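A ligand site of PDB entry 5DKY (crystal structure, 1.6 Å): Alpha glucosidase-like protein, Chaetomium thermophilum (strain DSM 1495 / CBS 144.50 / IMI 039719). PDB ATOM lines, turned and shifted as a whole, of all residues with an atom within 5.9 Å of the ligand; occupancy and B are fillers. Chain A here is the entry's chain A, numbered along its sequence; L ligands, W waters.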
ATOM      1  N   ASP A 277      30.930 -30.322 -31.467  1.00  0.00           N
ATOM      2  CA  ASP A 277      29.765 -29.621 -31.987  1.00  0.00           C
ATOM      3  C   ASP A 277      29.477 -30.167 -33.384  1.00  0.00           C
ATOM      4  O   ASP A 277      30.083 -29.715 -34.358  1.00  0.00           O
ATOM      5  CB  ASP A 277      30.029 -28.109 -32.014  1.00  0.00           C
ATOM      6  CG  ASP A 277      28.836 -27.287 -32.431  1.00  0.00           C
ATOM      7  OD1 ASP A 277      27.795 -27.870 -32.885  1.00  0.00           O
ATOM      8  OD2 ASP A 277      28.935 -26.035 -32.282  1.00  0.00           O
ATOM      9  N   TYR A 290      28.067 -34.662 -28.332  1.00  0.00           N
ATOM     10  CA  TYR A 290      28.458 -33.495 -27.512  1.00  0.00           C
ATOM     11  C   TYR A 290      28.980 -33.857 -26.122  1.00  0.00           C
ATOM     12  O   TYR A 290      29.702 -33.040 -25.515  1.00  0.00           O
ATOM     13  CB  TYR A 290      27.284 -32.497 -27.390  1.00  0.00           C
ATOM     14  CG  TYR A 290      26.595 -32.137 -28.674  1.00  0.00           C
ATOM     15  CD1 TYR A 290      26.988 -31.036 -29.430  1.00  0.00           C
ATOM     16  CD2 TYR A 290      25.495 -32.858 -29.095  1.00  0.00           C
ATOM     17  CE1 TYR A 290      26.286 -30.629 -30.568  1.00  0.00           C
ATOM     18  CE2 TYR A 290      24.846 -32.514 -30.276  1.00  0.00           C
ATOM     19  CZ  TYR A 290      25.210 -31.397 -31.000  1.00  0.00           C
ATOM     20  OH  TYR A 290      24.527 -31.039 -32.144  1.00  0.00           O
ATOM     21  N   TRP A 389      15.154 -20.395 -31.171  1.00  0.00           N
ATOM     22  CA  TRP A 389      16.202 -19.439 -31.532  1.00  0.00           C
ATOM     23  C   TRP A 389      15.547 -18.485 -32.555  1.00  0.00           C
ATOM     24  O   TRP A 389      15.452 -18.863 -33.747  1.00  0.00           O
ATOM     25  CB  TRP A 389      17.362 -20.194 -32.152  1.00  0.00           C
ATOM     26  CG  TRP A 389      18.575 -19.372 -32.572  1.00  0.00           C
ATOM     27  CD1 TRP A 389      18.793 -18.049 -32.315  1.00  0.00           C
ATOM     28  CD2 TRP A 389      19.694 -19.838 -33.323  1.00  0.00           C
ATOM     29  NE1 TRP A 389      19.994 -17.662 -32.843  1.00  0.00           N
ATOM     30  CE2 TRP A 389      20.582 -18.732 -33.466  1.00  0.00           C
ATOM     31  CE3 TRP A 389      20.056 -21.072 -33.866  1.00  0.00           C
ATOM     32  CZ2 TRP A 389      21.764 -18.832 -34.196  1.00  0.00           C
ATOM     33  CZ3 TRP A 389      21.240 -21.175 -34.554  1.00  0.00           C
ATOM     34  CH2 TRP A 389      22.107 -20.071 -34.703  1.00  0.00           C
ATOM     35  N   ASP A 417      17.483 -17.639 -26.172  1.00  0.00           N
ATOM     36  CA  ASP A 417      18.682 -17.948 -26.906  1.00  0.00           C
ATOM     37  C   ASP A 417      19.518 -16.684 -27.182  1.00  0.00           C
ATOM     38  O   ASP A 417      19.135 -15.594 -26.736  1.00  0.00           O
ATOM     39  CB  ASP A 417      18.273 -18.715 -28.189  1.00  0.00           C
ATOM     40  CG  ASP A 417      19.305 -19.765 -28.643  1.00  0.00           C
ATOM     41  OD1 ASP A 417      20.522 -19.530 -28.438  1.00  0.00           O
ATOM     42  OD2 ASP A 417      18.901 -20.767 -29.285  1.00  0.00           O
ATOM     43  N   ILE A 418      20.612 -16.839 -27.935  1.00  0.00           N
ATOM     44  CA  ILE A 418      21.750 -15.895 -27.966  1.00  0.00           C
ATOM     45  C   ILE A 418      21.390 -14.490 -28.467  1.00  0.00           C
ATOM     46  O   ILE A 418      22.134 -13.543 -28.177  1.00  0.00           O
ATOM     47  CB  ILE A 418      22.939 -16.389 -28.793  1.00  0.00           C
ATOM     48  CG1 ILE A 418      22.509 -16.844 -30.198  1.00  0.00           C
ATOM     49  CG2 ILE A 418      23.677 -17.505 -28.035  1.00  0.00           C
ATOM     50  CD1 ILE A 418      23.634 -17.268 -31.074  1.00  0.00           C
ATOM     51  N   ILE A 454      20.543 -18.040 -21.975  1.00  0.00           N
ATOM     52  CA  ILE A 454      21.772 -18.686 -22.404  1.00  0.00           C
ATOM     53  C   ILE A 454      23.021 -17.881 -22.011  1.00  0.00           C
ATOM     54  O   ILE A 454      23.030 -16.675 -22.089  1.00  0.00           O
ATOM     55  CB  ILE A 454      21.712 -19.023 -23.928  1.00  0.00           C
ATOM     56  CG1 ILE A 454      22.768 -20.078 -24.306  1.00  0.00           C
ATOM     57  CG2 ILE A 454      21.842 -17.800 -24.811  1.00  0.00           C
ATOM     58  CD1 ILE A 454      22.529 -20.620 -25.712  1.00  0.00           C
ATOM     59  N   ASP A 456      27.300 -18.774 -22.625  1.00  0.00           N
ATOM     60  CA  ASP A 456      28.269 -19.699 -23.188  1.00  0.00           C
ATOM     61  C   ASP A 456      29.675 -19.315 -22.673  1.00  0.00           C
ATOM     62  O   ASP A 456      29.834 -18.261 -22.031  1.00  0.00           O
ATOM     63  CB  ASP A 456      28.252 -19.599 -24.727  1.00  0.00           C
ATOM     64  CG  ASP A 456      26.941 -20.067 -25.345  1.00  0.00           C
ATOM     65  OD1 ASP A 456      26.096 -20.683 -24.659  1.00  0.00           O
ATOM     66  OD2 ASP A 456      26.830 -19.827 -26.592  1.00  0.00           O
ATOM     67  N   TRP A 491      30.250 -17.197 -31.716  1.00  0.00           N
ATOM     68  CA  TRP A 491      29.190 -16.205 -32.010  1.00  0.00           C
ATOM     69  C   TRP A 491      29.625 -14.758 -31.957  1.00  0.00           C
ATOM     70  O   TRP A 491      29.152 -13.958 -32.781  1.00  0.00           O
ATOM     71  CB  TRP A 491      27.961 -16.345 -31.113  1.00  0.00           C
ATOM     72  CG  TRP A 491      27.334 -17.632 -31.209  1.00  0.00           C
ATOM     73  CD1 TRP A 491      27.161 -18.526 -30.204  1.00  0.00           C
ATOM     74  CD2 TRP A 491      26.824 -18.234 -32.382  1.00  0.00           C
ATOM     75  NE1 TRP A 491      26.580 -19.647 -30.671  1.00  0.00           N
ATOM     76  CE2 TRP A 491      26.376 -19.517 -32.009  1.00  0.00           C
ATOM     77  CE3 TRP A 491      26.699 -17.838 -33.700  1.00  0.00           C
ATOM     78  CZ2 TRP A 491      25.810 -20.379 -32.903  1.00  0.00           C
ATOM     79  CZ3 TRP A 491      26.100 -18.740 -34.618  1.00  0.00           C
ATOM     80  CH2 TRP A 491      25.671 -19.966 -34.205  1.00  0.00           C
ATOM     81  N   TRP A 528      21.117 -21.555 -19.214  1.00  0.00           N
ATOM     82  CA  TRP A 528      21.426 -22.584 -20.213  1.00  0.00           C
ATOM     83  C   TRP A 528      22.890 -22.409 -20.612  1.00  0.00           C
ATOM     84  O   TRP A 528      23.251 -21.343 -21.100  1.00  0.00           O
ATOM     85  CB  TRP A 528      20.490 -22.380 -21.409  1.00  0.00           C
ATOM     86  CG  TRP A 528      20.715 -23.145 -22.624  1.00  0.00           C
ATOM     87  CD1 TRP A 528      21.456 -24.252 -22.795  1.00  0.00           C
ATOM     88  CD2 TRP A 528      20.098 -22.872 -23.884  1.00  0.00           C
ATOM     89  NE1 TRP A 528      21.381 -24.668 -24.112  1.00  0.00           N
ATOM     90  CE2 TRP A 528      20.546 -23.817 -24.797  1.00  0.00           C
ATOM     91  CE3 TRP A 528      19.231 -21.871 -24.341  1.00  0.00           C
ATOM     92  CZ2 TRP A 528      20.167 -23.811 -26.137  1.00  0.00           C
ATOM     93  CZ3 TRP A 528      18.846 -21.869 -25.647  1.00  0.00           C
ATOM     94  CH2 TRP A 528      19.310 -22.825 -26.532  1.00  0.00           C
ATOM     95  N   ASP A 530      25.676 -23.585 -23.221  1.00  0.00           N
ATOM     96  CA  ASP A 530      25.771 -24.188 -24.560  1.00  0.00           C
ATOM     97  C   ASP A 530      27.181 -24.026 -25.093  1.00  0.00           C
ATOM     98  O   ASP A 530      27.980 -23.309 -24.540  1.00  0.00           O
ATOM     99  CB  ASP A 530      24.690 -23.540 -25.436  1.00  0.00           C
ATOM    100  CG  ASP A 530      24.606 -24.087 -26.877  1.00  0.00           C
ATOM    101  OD1 ASP A 530      24.889 -25.256 -27.085  1.00  0.00           O
ATOM    102  OD2 ASP A 530      24.236 -23.272 -27.782  1.00  0.00           O
ATOM    103  N   MET A 531      27.493 -24.692 -26.212  1.00  0.00           N
ATOM    104  CA  MET A 531      28.783 -24.514 -26.909  1.00  0.00           C
ATOM    105  C   MET A 531      29.978 -24.802 -26.022  1.00  0.00           C
ATOM    106  O   MET A 531      31.092 -24.275 -26.265  1.00  0.00           O
ATOM    107  CB  MET A 531      28.915 -23.104 -27.515  1.00  0.00           C
ATOM    108  CG  MET A 531      27.689 -22.620 -28.249  1.00  0.00           C
ATOM    109  SD  MET A 531      27.248 -23.521 -29.748  1.00  0.00           S
ATOM    110  CE  MET A 531      28.412 -22.841 -30.896  1.00  0.00           C
ATOM    111  N   ARG A 591      25.056 -28.705 -22.754  1.00  0.00           N
ATOM    112  CA  ARG A 591      25.185 -29.508 -23.955  1.00  0.00           C
ATOM    113  C   ARG A 591      26.267 -30.559 -23.773  1.00  0.00           C
ATOM    114  O   ARG A 591      26.006 -31.734 -23.924  1.00  0.00           O
ATOM    115  CB  ARG A 591      25.397 -28.671 -25.194  1.00  0.00           C
ATOM    116  CG  ARG A 591      25.083 -29.460 -26.475  1.00  0.00           C
ATOM    117  CD  ARG A 591      25.050 -28.573 -27.700  1.00  0.00           C
ATOM    118  NE  ARG A 591      26.376 -28.078 -28.081  1.00  0.00           N
ATOM    119  CZ  ARG A 591      26.635 -27.438 -29.210  1.00  0.00           C
ATOM    120  NH1 ARG A 591      27.891 -27.089 -29.473  1.00  0.00           N
ATOM    121  NH2 ARG A 591      25.671 -27.085 -30.065  1.00  0.00           N
ATOM    122  N   TRP A 604      20.528 -32.031 -22.920  1.00  0.00           N
ATOM    123  CA  TRP A 604      19.725 -32.426 -24.071  1.00  0.00           C
ATOM    124  C   TRP A 604      20.634 -32.906 -25.184  1.00  0.00           C
ATOM    125  O   TRP A 604      21.812 -32.646 -25.188  1.00  0.00           O
ATOM    126  CB  TRP A 604      18.796 -31.286 -24.564  1.00  0.00           C
ATOM    127  CG  TRP A 604      19.362 -30.332 -25.566  1.00  0.00           C
ATOM    128  CD1 TRP A 604      18.959 -30.198 -26.895  1.00  0.00           C
ATOM    129  CD2 TRP A 604      20.411 -29.341 -25.398  1.00  0.00           C
ATOM    130  NE1 TRP A 604      19.681 -29.246 -27.505  1.00  0.00           N
ATOM    131  CE2 TRP A 604      20.552 -28.672 -26.619  1.00  0.00           C
ATOM    132  CE3 TRP A 604      21.182 -28.933 -24.316  1.00  0.00           C
ATOM    133  CZ2 TRP A 604      21.512 -27.686 -26.824  1.00  0.00           C
ATOM    134  CZ3 TRP A 604      22.108 -27.962 -24.499  1.00  0.00           C
ATOM    135  CH2 TRP A 604      22.272 -27.338 -25.761  1.00  0.00           C
ATOM    136  N   GLY A 606      21.207 -31.999 -28.206  1.00  0.00           N
ATOM    137  CA  GLY A 606      21.798 -31.078 -29.162  1.00  0.00           C
ATOM    138  C   GLY A 606      20.955 -30.904 -30.399  1.00  0.00           C
ATOM    139  O   GLY A 606      19.707 -30.983 -30.334  1.00  0.00           O
ATOM    140  N   ASP A 607      21.623 -30.666 -31.528  1.00  0.00           N
ATOM    141  CA  ASP A 607      20.958 -30.229 -32.750  1.00  0.00           C
ATOM    142  C   ASP A 607      20.422 -31.419 -33.545  1.00  0.00           C
ATOM    143  O   ASP A 607      20.985 -31.802 -34.565  1.00  0.00           O
ATOM    144  CB  ASP A 607      21.897 -29.332 -33.580  1.00  0.00           C
ATOM    145  CG  ASP A 607      22.240 -28.051 -32.841  1.00  0.00           C
ATOM    146  OD1 ASP A 607      21.554 -27.672 -31.881  1.00  0.00           O
ATOM    147  OD2 ASP A 607      23.203 -27.389 -33.258  1.00  0.00           O
ATOM    148  N   ASP A 636      15.218 -32.050 -28.298  1.00  0.00           N
ATOM    149  CA  ASP A 636      14.362 -30.893 -28.693  1.00  0.00           C
ATOM    150  C   ASP A 636      13.061 -31.400 -29.322  1.00  0.00           C
ATOM    151  O   ASP A 636      13.079 -32.083 -30.373  1.00  0.00           O
ATOM    152  CB  ASP A 636      15.089 -30.006 -29.707  1.00  0.00           C
ATOM    153  CG  ASP A 636      16.220 -29.237 -29.113  1.00  0.00           C
ATOM    154  OD1 ASP A 636      16.272 -29.099 -27.861  1.00  0.00           O
ATOM    155  OD2 ASP A 636      17.038 -28.704 -29.918  1.00  0.00           O
ATOM    156  N   PHE A 640      15.293 -29.749 -33.819  1.00  0.00           N
ATOM    157  CA  PHE A 640      15.932 -28.443 -33.928  1.00  0.00           C
ATOM    158  C   PHE A 640      15.908 -27.938 -35.384  1.00  0.00           C
ATOM    159  O   PHE A 640      15.327 -26.882 -35.649  1.00  0.00           O
ATOM    160  CB  PHE A 640      17.320 -28.535 -33.395  1.00  0.00           C
ATOM    161  CG  PHE A 640      18.092 -27.273 -33.470  1.00  0.00           C
ATOM    162  CD1 PHE A 640      17.802 -26.210 -32.625  1.00  0.00           C
ATOM    163  CD2 PHE A 640      19.138 -27.158 -34.362  1.00  0.00           C
ATOM    164  CE1 PHE A 640      18.567 -25.039 -32.694  1.00  0.00           C
ATOM    165  CE2 PHE A 640      19.919 -25.998 -34.403  1.00  0.00           C
ATOM    166  CZ  PHE A 640      19.618 -24.957 -33.545  1.00  0.00           C
ATOM    167  N   ARG A 663      11.630 -30.050 -23.323  1.00  0.00           N
ATOM    168  CA  ARG A 663      11.675 -28.722 -23.982  1.00  0.00           C
ATOM    169  C   ARG A 663      11.430 -28.774 -25.467  1.00  0.00           C
ATOM    170  O   ARG A 663      12.025 -29.605 -26.171  1.00  0.00           O
ATOM    171  CB  ARG A 663      13.083 -28.113 -23.746  1.00  0.00           C
ATOM    172  CG  ARG A 663      13.346 -26.777 -24.420  1.00  0.00           C
ATOM    173  CD  ARG A 663      14.771 -26.272 -24.130  1.00  0.00           C
ATOM    174  NE  ARG A 663      15.740 -26.961 -24.985  1.00  0.00           N
ATOM    175  CZ  ARG A 663      16.885 -26.463 -25.437  1.00  0.00           C
ATOM    176  NH1 ARG A 663      17.332 -25.287 -25.031  1.00  0.00           N
ATOM    177  NH2 ARG A 663      17.622 -27.180 -26.293  1.00  0.00           N
ATOM    178  N   HIS A 665      12.137 -26.690 -28.952  1.00  0.00           N
ATOM    179  CA  HIS A 665      13.170 -25.766 -29.428  1.00  0.00           C
ATOM    180  C   HIS A 665      13.242 -25.892 -30.946  1.00  0.00           C
ATOM    181  O   HIS A 665      12.829 -26.913 -31.490  1.00  0.00           O
ATOM    182  CB  HIS A 665      14.496 -26.098 -28.741  1.00  0.00           C
ATOM    183  CG  HIS A 665      15.625 -25.159 -29.071  1.00  0.00           C
ATOM    184  ND1 HIS A 665      15.435 -23.808 -29.271  1.00  0.00           N
ATOM    185  CD2 HIS A 665      16.943 -25.370 -29.212  1.00  0.00           C
ATOM    186  CE1 HIS A 665      16.595 -23.236 -29.518  1.00  0.00           C
ATOM    187  NE2 HIS A 665      17.528 -24.165 -29.484  1.00  0.00           N
ATOM    188  N   ALA A 666      13.741 -24.833 -31.596  1.00  0.00           N
ATOM    189  CA  ALA A 666      13.761 -24.717 -33.043  1.00  0.00           C
ATOM    190  C   ALA A 666      14.910 -23.807 -33.496  1.00  0.00           C
ATOM    191  O   ALA A 666      15.180 -22.813 -32.871  1.00  0.00           O
ATOM    192  CB  ALA A 666      12.438 -24.151 -33.525  1.00  0.00           C
ATOM    193  N   HIS A 667      15.488 -24.150 -34.620  1.00  0.00           N
ATOM    194  CA  HIS A 667      16.605 -23.449 -35.231  1.00  0.00           C
ATOM    195  C   HIS A 667      16.092 -22.120 -35.804  1.00  0.00           C
ATOM    196  O   HIS A 667      14.894 -21.960 -36.027  1.00  0.00           O
ATOM    197  CB  HIS A 667      17.211 -24.390 -36.285  1.00  0.00           C
ATOM    198  CG  HIS A 667      18.204 -23.774 -37.204  1.00  0.00           C
ATOM    199  ND1 HIS A 667      19.546 -23.666 -36.929  1.00  0.00           N
ATOM    200  CD2 HIS A 667      18.037 -23.267 -38.448  1.00  0.00           C
ATOM    201  CE1 HIS A 667      20.170 -23.098 -37.951  1.00  0.00           C
ATOM    202  NE2 HIS A 667      19.273 -22.834 -38.880  1.00  0.00           N
HETATM  203  C1  LIG L   1      23.677 -24.625 -30.449  1.00  0.00           C
HETATM  204  C2  LIG L   1      22.577 -25.273 -29.621  1.00  0.00           C
HETATM  205  O1  LIG L   1      22.728 -26.710 -29.746  1.00  0.00           O
HETATM  206  C3  LIG L   1      21.217 -24.763 -30.064  1.00  0.00           C
HETATM  207  O2  LIG L   1      20.213 -25.256 -29.191  1.00  0.00           O
HETATM  208  C4  LIG L   1      21.217 -23.215 -30.042  1.00  0.00           C
HETATM  209  O3  LIG L   1      19.941 -22.780 -30.488  1.00  0.00           O
HETATM  210  C5  LIG L   1      22.305 -22.624 -30.932  1.00  0.00           C
HETATM  211  N1  LIG L   1      23.554 -23.152 -30.486  1.00  0.00           N
HETATM  212  C6  LIG L   1      22.377 -21.107 -30.958  1.00  0.00           C
HETATM  213  O4  LIG L   1      22.550 -20.647 -29.599  1.00  0.00           O
HETATM  214  O   HOH W   1      25.131 -23.309 -32.905  1.00  0.00           O
HETATM  215  O   HOH W   2      25.860 -25.976 -32.615  1.00  0.00           O
HETATM  216  O   HOH W   3      25.021 -20.750 -28.101  1.00  0.00           O
HETATM  217  O   HOH W   4      19.435 -27.795 -29.967  1.00  0.00           O
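Water W3 lies within hydrogen-bond range of OD2 of Asp 456 (2.5 Å), OD2 of Asp 530 (2.7 Å), O4 of the ligand (2.9 Å) and NE1 of Trp 491 (3.2 Å). Water W2 lies within hydrogen-bond range of the side-chain carboxylate of Asp 277 (2.7 Å), the guanidinium group of Arg 591 (2.8 Å) and the side-chain carboxylate of Asp 607 (3.1 Å).
O1 of the ligand sits at hydrogen-bond distance from NH2 of Arg 591, 3.0 Å away. OD1 of Asp 607 is in hydrogen-bond range of O1 of the ligand (2.6 Å). SD of Met 531 is in hydrogen-bond range of N1 of the ligand, 3.8 Å away. An oxygen (O2) of the ligand lies within hydrogen-bond range of a ring nitrogen (NE2) of His 665. OD2 of Asp 530 is in salt-bridge range of N1 of the ligand. O3 of the ligand is in hydrogen-bond range of OD2 of Asp 417 (2.6 Å).
The backbone carbonyl oxygen (O) of Ala 666 lies within hydrogen-bond range of the backbone NH (N) of Trp 389. The backbone carbonyl oxygen (O) of Phe 640 is in hydrogen-bond range of the backbone NH (N) of His 667 (2.9 Å). The side-chain carboxylate (OD1) of Asp 530 is in salt-bridge range of the guanidinium group (NE) of Arg 591 (3.3 Å). The side-chain carboxylate (OD1) of Asp 636 sits close to the indole nitrogen (NE1) of Trp 604, 3.4 Å away. N of Asp 607 lies within hydrogen-bond range of OH of Tyr 290, 3.0 Å away. SD of Met 531 is in hydrogen-bond range of NH1 of Arg 591, 3.6 Å away. The backbone NH of Asp 530 lies within hydrogen-bond range of the side-chain carboxylate of Asp 456 (3.3 Å). The guanidinium group (NH1) of Arg 591 is in salt-bridge range of the side-chain carboxylate (OD2) of Asp 277 (3.2 Å).
CE3 of Trp 389 touches C6 of the ligand, at 3.7 Å. Ile 418 touches the ligand. Ile 454 touches the ligand (CD1 to O4, 3.9 Å). CZ2 of Trp 528 touches O2 of the ligand (3.4 Å). Trp 604 touches the ligand. Phe 640 touches the ligand (CE1 to O3, 3.4 Å). Hydrophobic or aromatic side chains within 4 Å of the ligand: Trp 389, Ile 418, Ile 454, Trp 528, Met 531, Trp 604, Phe 640 and His 665. Within 4 Å of the ligand: Trp 389, Asp 417, Ile 418, Ile 454, Trp 528, Asp 530, Met 531, Arg 591, Trp 604, Asp 607, Phe 640 and His 665.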
